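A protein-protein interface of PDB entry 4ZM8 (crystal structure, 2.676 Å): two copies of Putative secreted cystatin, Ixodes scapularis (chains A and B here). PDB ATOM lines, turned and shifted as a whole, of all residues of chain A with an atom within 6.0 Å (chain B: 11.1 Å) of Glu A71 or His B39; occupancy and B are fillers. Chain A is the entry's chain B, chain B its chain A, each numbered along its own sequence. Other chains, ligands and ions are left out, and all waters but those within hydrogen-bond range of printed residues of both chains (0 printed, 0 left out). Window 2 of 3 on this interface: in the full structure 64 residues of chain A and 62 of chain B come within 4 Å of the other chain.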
ATOM      1  N   GLU A  67      32.589  -8.292  -0.574  1.00  0.00           N
ATOM      2  CA  GLU A  67      31.223  -7.923  -0.939  1.00  0.00           C
ATOM      3  C   GLU A  67      30.614  -7.133   0.209  1.00  0.00           C
ATOM      4  O   GLU A  67      30.703  -7.556   1.358  1.00  0.00           O
ATOM      5  CB  GLU A  67      30.389  -9.181  -1.250  1.00  0.00           C
ATOM      6  CG  GLU A  67      29.033  -8.963  -1.977  1.00  0.00           C
ATOM      7  CD  GLU A  67      28.234 -10.271  -2.229  1.00  0.00           C
ATOM      8  OE1 GLU A  67      27.032 -10.178  -2.570  1.00  0.00           O
ATOM      9  OE2 GLU A  67      28.790 -11.387  -2.089  1.00  0.00           O
ATOM     10  N   SER A  68      30.031  -5.974  -0.093  1.00  0.00           N
ATOM     11  CA  SER A  68      29.372  -5.148   0.922  1.00  0.00           C
ATOM     12  C   SER A  68      27.868  -5.440   1.035  1.00  0.00           C
ATOM     13  O   SER A  68      27.334  -6.258   0.299  1.00  0.00           O
ATOM     14  CB  SER A  68      29.559  -3.664   0.611  1.00  0.00           C
ATOM     15  OG  SER A  68      28.627  -3.276  -0.381  1.00  0.00           O
ATOM     16  N   THR A  69      27.192  -4.749   1.949  1.00  0.00           N
ATOM     17  CA  THR A  69      25.748  -4.924   2.132  1.00  0.00           C
ATOM     18  C   THR A  69      24.868  -4.139   1.129  1.00  0.00           C
ATOM     19  O   THR A  69      23.674  -4.422   0.977  1.00  0.00           O
ATOM     20  CB  THR A  69      25.336  -4.514   3.545  1.00  0.00           C
ATOM     21  OG1 THR A  69      25.688  -3.141   3.780  1.00  0.00           O
ATOM     22  CG2 THR A  69      26.040  -5.376   4.547  1.00  0.00           C
ATOM     23  N   CYS A  70      25.470  -3.167   0.446  1.00  0.00           N
ATOM     24  CA  CYS A  70      24.743  -2.252  -0.432  1.00  0.00           C
ATOM     25  C   CYS A  70      24.565  -2.765  -1.857  1.00  0.00           C
ATOM     26  O   CYS A  70      25.411  -3.468  -2.391  1.00  0.00           O
ATOM     27  CB  CYS A  70      25.452  -0.903  -0.486  1.00  0.00           C
ATOM     28  SG  CYS A  70      25.332   0.043   1.018  1.00  0.00           S
ATOM     29  N   GLU A  71      23.469  -2.393  -2.493  1.00  0.00           N
ATOM     30  CA  GLU A  71      23.295  -2.804  -3.869  1.00  0.00           C
ATOM     31  C   GLU A  71      23.868  -1.733  -4.766  1.00  0.00           C
ATOM     32  O   GLU A  71      23.976  -0.574  -4.370  1.00  0.00           O
ATOM     33  CB  GLU A  71      21.828  -3.055  -4.186  1.00  0.00           C
ATOM     34  CG  GLU A  71      21.171  -3.996  -3.217  1.00  0.00           C
ATOM     35  CD  GLU A  71      20.293  -5.006  -3.910  1.00  0.00           C
ATOM     36  OE1 GLU A  71      20.847  -5.913  -4.566  1.00  0.00           O
ATOM     37  OE2 GLU A  71      19.055  -4.897  -3.802  1.00  0.00           O
ATOM     38  N   LEU A  72      24.237  -2.126  -5.979  1.00  0.00           N
ATOM     39  CA  LEU A  72      24.764  -1.184  -6.942  1.00  0.00           C
ATOM     40  C   LEU A  72      23.718  -0.110  -7.239  1.00  0.00           C
ATOM     41  O   LEU A  72      24.054   1.026  -7.592  1.00  0.00           O
ATOM     42  CB  LEU A  72      25.202  -1.910  -8.216  1.00  0.00           C
ATOM     43  CG  LEU A  72      26.540  -2.631  -8.079  1.00  0.00           C
ATOM     44  CD1 LEU A  72      26.966  -3.290  -9.379  1.00  0.00           C
ATOM     45  CD2 LEU A  72      27.608  -1.651  -7.575  1.00  0.00           C
ATOM     46  N   THR A  73      22.450  -0.461  -7.061  1.00  0.00           N
ATOM     47  CA  THR A  73      21.365   0.480  -7.321  1.00  0.00           C
ATOM     48  C   THR A  73      21.336   1.624  -6.308  1.00  0.00           C
ATOM     49  O   THR A  73      20.663   2.629  -6.530  1.00  0.00           O
ATOM     50  CB  THR A  73      20.009  -0.223  -7.308  1.00  0.00           C
ATOM     51  OG1 THR A  73      19.784  -0.762  -6.006  1.00  0.00           O
ATOM     52  CG2 THR A  73      19.987  -1.358  -8.314  1.00  0.00           C
ATOM     53  N   SER A  74      22.070   1.479  -5.206  1.00  0.00           N
ATOM     54  CA  SER A  74      22.002   2.471  -4.136  1.00  0.00           C
ATOM     55  C   SER A  74      23.256   3.338  -4.095  1.00  0.00           C
ATOM     56  O   SER A  74      24.253   3.033  -4.732  1.00  0.00           O
ATOM     57  CB  SER A  74      21.790   1.793  -2.771  1.00  0.00           C
ATOM     58  OG  SER A  74      23.022   1.502  -2.116  1.00  0.00           O
ATOM     59  N   THR A  75      23.198   4.428  -3.346  1.00  0.00           N
ATOM     60  CA  THR A  75      24.340   5.312  -3.229  1.00  0.00           C
ATOM     61  C   THR A  75      25.266   4.777  -2.163  1.00  0.00           C
ATOM     62  O   THR A  75      24.830   4.524  -1.035  1.00  0.00           O
ATOM     63  CB  THR A  75      23.930   6.732  -2.870  1.00  0.00           C
ATOM     64  OG1 THR A  75      23.004   7.219  -3.851  1.00  0.00           O
ATOM     65  CG2 THR A  75      25.160   7.628  -2.829  1.00  0.00           C
ATOM     66  N   LYS A  84      29.936  -7.676   4.396  1.00  0.00           N
ATOM     67  CA  LYS A  84      29.162  -8.858   4.708  1.00  0.00           C
ATOM     68  C   LYS A  84      29.975  -9.892   5.502  1.00  0.00           C
ATOM     69  O   LYS A  84      31.043 -10.322   5.052  1.00  0.00           O
ATOM     70  CB  LYS A  84      28.654  -9.470   3.406  1.00  0.00           C
ATOM     71  CG  LYS A  84      27.293 -10.084   3.502  1.00  0.00           C
ATOM     72  CD  LYS A  84      26.693 -10.306   2.128  1.00  0.00           C
ATOM     73  CE  LYS A  84      26.541  -8.984   1.395  1.00  0.00           C
ATOM     74  NZ  LYS A  84      25.980  -9.127   0.024  1.00  0.00           N
ATOM     75  N   ALA B  26      38.207   4.376  -3.814  1.00  0.00           N
ATOM     76  CA  ALA B  26      38.745   3.470  -4.819  1.00  0.00           C
ATOM     77  C   ALA B  26      37.911   2.203  -4.975  1.00  0.00           C
ATOM     78  O   ALA B  26      37.648   1.775  -6.087  1.00  0.00           O
ATOM     79  CB  ALA B  26      40.184   3.099  -4.479  1.00  0.00           C
ATOM     80  N   THR B  27      37.514   1.601  -3.857  1.00  0.00           N
ATOM     81  CA  THR B  27      36.796   0.325  -3.876  1.00  0.00           C
ATOM     82  C   THR B  27      35.374   0.443  -4.406  1.00  0.00           C
ATOM     83  O   THR B  27      34.932  -0.380  -5.213  1.00  0.00           O
ATOM     84  CB  THR B  27      36.717  -0.306  -2.480  1.00  0.00           C
ATOM     85  OG1 THR B  27      38.034  -0.418  -1.926  1.00  0.00           O
ATOM     86  CG2 THR B  27      36.121  -1.679  -2.580  1.00  0.00           C
ATOM     87  N   SER B  28      34.654   1.452  -3.932  1.00  0.00           N
ATOM     88  CA  SER B  28      33.282   1.669  -4.359  1.00  0.00           C
ATOM     89  C   SER B  28      33.229   1.936  -5.849  1.00  0.00           C
ATOM     90  O   SER B  28      32.432   1.329  -6.569  1.00  0.00           O
ATOM     91  CB  SER B  28      32.668   2.835  -3.592  1.00  0.00           C
ATOM     92  OG  SER B  28      33.434   4.014  -3.759  1.00  0.00           O
ATOM     93  N   THR B  29      34.099   2.848  -6.289  1.00  0.00           N
ATOM     94  CA  THR B  29      34.238   3.273  -7.683  1.00  0.00           C
ATOM     95  C   THR B  29      34.574   2.136  -8.634  1.00  0.00           C
ATOM     96  O   THR B  29      33.958   1.996  -9.691  1.00  0.00           O
ATOM     97  CB  THR B  29      35.342   4.326  -7.808  1.00  0.00           C
ATOM     98  OG1 THR B  29      35.026   5.449  -6.981  1.00  0.00           O
ATOM     99  CG2 THR B  29      35.526   4.768  -9.254  1.00  0.00           C
ATOM    100  N   TRP B  30      35.560   1.327  -8.260  1.00  0.00           N
ATOM    101  CA  TRP B  30      36.037   0.286  -9.144  1.00  0.00           C
ATOM    102  C   TRP B  30      35.011  -0.830  -9.318  1.00  0.00           C
ATOM    103  O   TRP B  30      34.693  -1.201 -10.438  1.00  0.00           O
ATOM    104  CB  TRP B  30      37.363  -0.284  -8.639  1.00  0.00           C
ATOM    105  CG  TRP B  30      37.804  -1.468  -9.440  1.00  0.00           C
ATOM    106  CD1 TRP B  30      38.381  -1.454 -10.679  1.00  0.00           C
ATOM    107  CD2 TRP B  30      37.687  -2.844  -9.067  1.00  0.00           C
ATOM    108  NE1 TRP B  30      38.635  -2.738 -11.095  1.00  0.00           N
ATOM    109  CE2 TRP B  30      38.218  -3.612 -10.122  1.00  0.00           C
ATOM    110  CE3 TRP B  30      37.192  -3.503  -7.941  1.00  0.00           C
ATOM    111  CZ2 TRP B  30      38.259  -4.995 -10.087  1.00  0.00           C
ATOM    112  CZ3 TRP B  30      37.233  -4.886  -7.909  1.00  0.00           C
ATOM    113  CH2 TRP B  30      37.759  -5.614  -8.972  1.00  0.00           C
ATOM    114  N   SER B  31      34.483  -1.348  -8.213  1.00  0.00           N
ATOM    115  CA  SER B  31      33.601  -2.521  -8.239  1.00  0.00           C
ATOM    116  C   SER B  31      32.230  -2.247  -8.866  1.00  0.00           C
ATOM    117  O   SER B  31      31.575  -3.169  -9.361  1.00  0.00           O
ATOM    118  CB  SER B  31      33.420  -3.060  -6.825  1.00  0.00           C
ATOM    119  OG  SER B  31      32.839  -2.063  -6.006  1.00  0.00           O
ATOM    120  N   ALA B  32      31.809  -0.982  -8.824  1.00  0.00           N
ATOM    121  CA  ALA B  32      30.609  -0.516  -9.514  1.00  0.00           C
ATOM    122  C   ALA B  32      30.683  -0.826 -10.994  1.00  0.00           C
ATOM    123  O   ALA B  32      29.788  -1.437 -11.561  1.00  0.00           O
ATOM    124  CB  ALA B  32      30.433   0.967  -9.305  1.00  0.00           C
ATOM    125  N   GLN B  33      31.779  -0.415 -11.612  1.00  0.00           N
ATOM    126  CA  GLN B  33      32.020  -0.675 -13.022  1.00  0.00           C
ATOM    127  C   GLN B  33      32.244  -2.151 -13.344  1.00  0.00           C
ATOM    128  O   GLN B  33      32.340  -2.514 -14.505  1.00  0.00           O
ATOM    129  CB  GLN B  33      33.224   0.134 -13.490  1.00  0.00           C
ATOM    130  CG  GLN B  33      33.174   1.589 -13.072  1.00  0.00           C
ATOM    131  CD  GLN B  33      34.555   2.218 -13.030  1.00  0.00           C
ATOM    132  OE1 GLN B  33      35.575   1.521 -13.122  1.00  0.00           O
ATOM    133  NE2 GLN B  33      34.598   3.540 -12.859  1.00  0.00           N
ATOM    134  N   GLN B  34      32.327  -3.008 -12.335  1.00  0.00           N
ATOM    135  CA  GLN B  34      32.540  -4.437 -12.590  1.00  0.00           C
ATOM    136  C   GLN B  34      31.258  -5.176 -12.973  1.00  0.00           C
ATOM    137  O   GLN B  34      30.163  -4.886 -12.447  1.00  0.00           O
ATOM    138  CB  GLN B  34      33.173  -5.111 -11.377  1.00  0.00           C
ATOM    139  CG  GLN B  34      34.512  -4.518 -11.010  1.00  0.00           C
ATOM    140  CD  GLN B  34      35.551  -4.705 -12.095  1.00  0.00           C
ATOM    141  OE1 GLN B  34      36.186  -5.764 -12.193  1.00  0.00           O
ATOM    142  NE2 GLN B  34      35.730  -3.678 -12.924  1.00  0.00           N
ATOM    143  N   PRO B  35      31.401  -6.136 -13.906  1.00  0.00           N
ATOM    144  CA  PRO B  35      30.322  -6.952 -14.470  1.00  0.00           C
ATOM    145  C   PRO B  35      30.078  -8.202 -13.652  1.00  0.00           C
ATOM    146  O   PRO B  35      31.030  -8.751 -13.098  1.00  0.00           O
ATOM    147  CB  PRO B  35      30.851  -7.304 -15.858  1.00  0.00           C
ATOM    148  CG  PRO B  35      32.331  -7.394 -15.663  1.00  0.00           C
ATOM    149  CD  PRO B  35      32.688  -6.397 -14.578  1.00  0.00           C
ATOM    150  N   GLY B  36      28.825  -8.643 -13.587  1.00  0.00           N
ATOM    151  CA  GLY B  36      28.452  -9.766 -12.745  1.00  0.00           C
ATOM    152  C   GLY B  36      28.081  -9.260 -11.361  1.00  0.00           C
ATOM    153  O   GLY B  36      27.065  -9.658 -10.782  1.00  0.00           O
ATOM    154  N   LYS B  37      28.915  -8.365 -10.842  1.00  0.00           N
ATOM    155  CA  LYS B  37      28.715  -7.768  -9.530  1.00  0.00           C
ATOM    156  C   LYS B  37      27.327  -7.148  -9.415  1.00  0.00           C
ATOM    157  O   LYS B  37      26.879  -6.453 -10.321  1.00  0.00           O
ATOM    158  CB  LYS B  37      29.789  -6.707  -9.267  1.00  0.00           C
ATOM    159  CG  LYS B  37      30.744  -7.028  -8.121  1.00  0.00           C
ATOM    160  CD  LYS B  37      31.563  -8.287  -8.372  1.00  0.00           C
ATOM    161  CE  LYS B  37      32.476  -8.640  -7.185  1.00  0.00           C
ATOM    162  NZ  LYS B  37      31.726  -9.123  -5.966  1.00  0.00           N
ATOM    163  N   THR B  38      26.643  -7.415  -8.306  1.00  0.00           N
ATOM    164  CA  THR B  38      25.370  -6.763  -8.013  1.00  0.00           C
ATOM    165  C   THR B  38      25.490  -5.809  -6.822  1.00  0.00           C
ATOM    166  O   THR B  38      24.767  -4.818  -6.743  1.00  0.00           O
ATOM    167  CB  THR B  38      24.271  -7.782  -7.726  1.00  0.00           C
ATOM    168  OG1 THR B  38      24.674  -8.608  -6.631  1.00  0.00           O
ATOM    169  CG2 THR B  38      24.029  -8.649  -8.946  1.00  0.00           C
ATOM    170  N   HIS B  39      26.406  -6.112  -5.902  1.00  0.00           N
ATOM    171  CA  HIS B  39      26.671  -5.253  -4.740  1.00  0.00           C
ATOM    172  C   HIS B  39      27.975  -4.468  -4.873  1.00  0.00           C
ATOM    173  O   HIS B  39      28.856  -4.832  -5.660  1.00  0.00           O
ATOM    174  CB  HIS B  39      26.724  -6.091  -3.455  1.00  0.00           C
ATOM    175  CG  HIS B  39      25.410  -6.689  -3.065  1.00  0.00           C
ATOM    176  ND1 HIS B  39      24.734  -7.585  -3.865  1.00  0.00           N
ATOM    177  CD2 HIS B  39      24.641  -6.520  -1.963  1.00  0.00           C
ATOM    178  CE1 HIS B  39      23.609  -7.941  -3.273  1.00  0.00           C
ATOM    179  NE2 HIS B  39      23.529  -7.311  -2.115  1.00  0.00           N
ATOM    180  N   PHE B  40      28.111  -3.408  -4.085  1.00  0.00           N
ATOM    181  CA  PHE B  40      29.417  -2.773  -3.938  1.00  0.00           C
ATOM    182  C   PHE B  40      30.370  -3.689  -3.186  1.00  0.00           C
ATOM    183  O   PHE B  40      29.948  -4.452  -2.305  1.00  0.00           O
ATOM    184  CB  PHE B  40      29.322  -1.444  -3.186  1.00  0.00           C
ATOM    185  CG  PHE B  40      28.584  -0.388  -3.927  1.00  0.00           C
ATOM    186  CD1 PHE B  40      29.194   0.302  -4.954  1.00  0.00           C
ATOM    187  CD2 PHE B  40      27.274  -0.084  -3.602  1.00  0.00           C
ATOM    188  CE1 PHE B  40      28.510   1.275  -5.639  1.00  0.00           C
ATOM    189  CE2 PHE B  40      26.589   0.887  -4.285  1.00  0.00           C
ATOM    190  CZ  PHE B  40      27.209   1.565  -5.304  1.00  0.00           C
ATOM    191  N   ASP B  41      31.645  -3.634  -3.551  1.00  0.00           N
ATOM    192  CA  ASP B  41      32.712  -4.147  -2.703  1.00  0.00           C
ATOM    193  C   ASP B  41      33.011  -3.054  -1.707  1.00  0.00           C
ATOM    194  O   ASP B  41      32.751  -1.880  -1.982  1.00  0.00           O
ATOM    195  CB  ASP B  41      33.968  -4.482  -3.497  1.00  0.00           C
ATOM    196  CG  ASP B  41      33.895  -5.822  -4.174  1.00  0.00           C
ATOM    197  OD1 ASP B  41      32.956  -6.593  -3.857  1.00  0.00           O
ATOM    198  OD2 ASP B  41      34.788  -6.101  -5.009  1.00  0.00           O
ATOM    199  N   THR B  42      33.550  -3.417  -0.555  1.00  0.00           N
ATOM    200  CA  THR B  42      33.958  -2.392   0.396  1.00  0.00           C
ATOM    201  C   THR B  42      35.300  -2.743   1.041  1.00  0.00           C
ATOM    202  O   THR B  42      35.963  -3.717   0.672  1.00  0.00           O
ATOM    203  CB  THR B  42      32.886  -2.166   1.479  1.00  0.00           C
ATOM    204  OG1 THR B  42      33.139  -0.928   2.158  1.00  0.00           O
ATOM    205  CG2 THR B  42      32.878  -3.320   2.476  1.00  0.00           C
ATOM    206  N   VAL B  43      35.725  -1.918   1.980  1.00  0.00           N
ATOM    207  CA  VAL B  43      36.979  -2.184   2.644  1.00  0.00           C
ATOM    208  C   VAL B  43      36.771  -3.013   3.916  1.00  0.00           C
ATOM    209  O   VAL B  43      36.114  -2.574   4.863  1.00  0.00           O
ATOM    210  CB  VAL B  43      37.684  -0.885   2.972  1.00  0.00           C
ATOM    211  CG1 VAL B  43      39.067  -1.155   3.565  1.00  0.00           C
ATOM    212  CG2 VAL B  43      37.775  -0.025   1.712  1.00  0.00           C
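No position is printed for both chains. Of the 19 pairs that touch across the chains among the printed residues, none has its exchanged pair printed and touching as well.
Thr A69 touches one residue of chain B. Of chain B, only His B39 and Phe B40 come within 4 Å of Cys A70. Glu A71 touches three residues of chain B. Ser A74 touches just one residue of chain B: Phe B40 (3.2 Å). Of the printed residues of chain B, Lys A84 touches His B39. Of the printed residues of chain A, Thr B38 touches Glu A71 and Leu A72. Of chain A, only Glu A67 (3.7 Å), Ser A68 (3.5 Å), Thr A69 (3.7 Å), Cys A70 (3.1 Å), Glu A71 (3.7 Å), Leu A72 (3.9 Å) and Lys A84 (3.5 Å) come within 4 Å of His B39. Printed residues of chain A within 4 Å of Phe B40: Glu A67, Ser A68, Cys A70, Glu A71, Leu A72 and Ser A74. Of the printed residues of chain A, Thr B42 touches Ser A68. The nearest residue of chain B that does not touch Glu A71 is Lys B37 (7.9 Å). The nearest printed residue of chain A that does not touch His B39 is Thr A73 (6.8 Å).
Among the printed residues, merely in contact across the chains: Glu A67 with His B39, Glu A67 with Phe B40, Glu A67 with Asp B41, Ser A68 with His B39, Ser A68 with Thr B42, Thr A69 with His B39, Cys A70 with His B39, Glu A71 with Thr B38, Glu A71 with His B39, Glu A71 with Phe B40, Leu A72 with Ala B32, Leu A72 with Lys B37, Leu A72 with His B39, Leu A72 with Phe B40, Ser A74 with Phe B40 and Lys A84 with His B39.
Of the 18 printed residues of chain B, 7 touch a printed residue of chain A. Hydrophobic or aromatic side chains of chain B within 4 Å of the printed part of chain A: His B39 and Phe B40.
N of Leu A72 lies within hydrogen-bond range of O of Thr B38 (2.8 Å). O of Phe B40 lies within hydrogen-bond range of OG of Ser A68. The backbone NH (N) of Phe B40 is in hydrogen-bond range of the backbone carbonyl oxygen (O) of Cys A70, 3.2 Å away.
The backbone NH of Asp B41 sits at hydrogen-bond distance from the side-chain hydroxyl of Ser B31, 3.1 Å away. The side-chain carboxylate (OE1) of Glu A67 lies within salt-bridge range of the side-chain amino group (NZ) of Lys A84 (3.0 Å). The backbone carbonyl oxygen (O) of Ser A68 lies close to the side-chain amino group (NZ) of Lys A84 (3.2 Å). A ring nitrogen (ND1) of His B39 sits at hydrogen-bond distance from the side-chain hydroxyl (OG1) of Thr B38. The backbone NH (N) of Cys A70 is in hydrogen-bond range of the side-chain hydroxyl (OG) of Ser A68 (3.3 Å). The side-chain amino group (NZ) of Lys B37 is in salt-bridge range of the side-chain carboxylate (OD1) of Asp B41 (3.5 Å).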
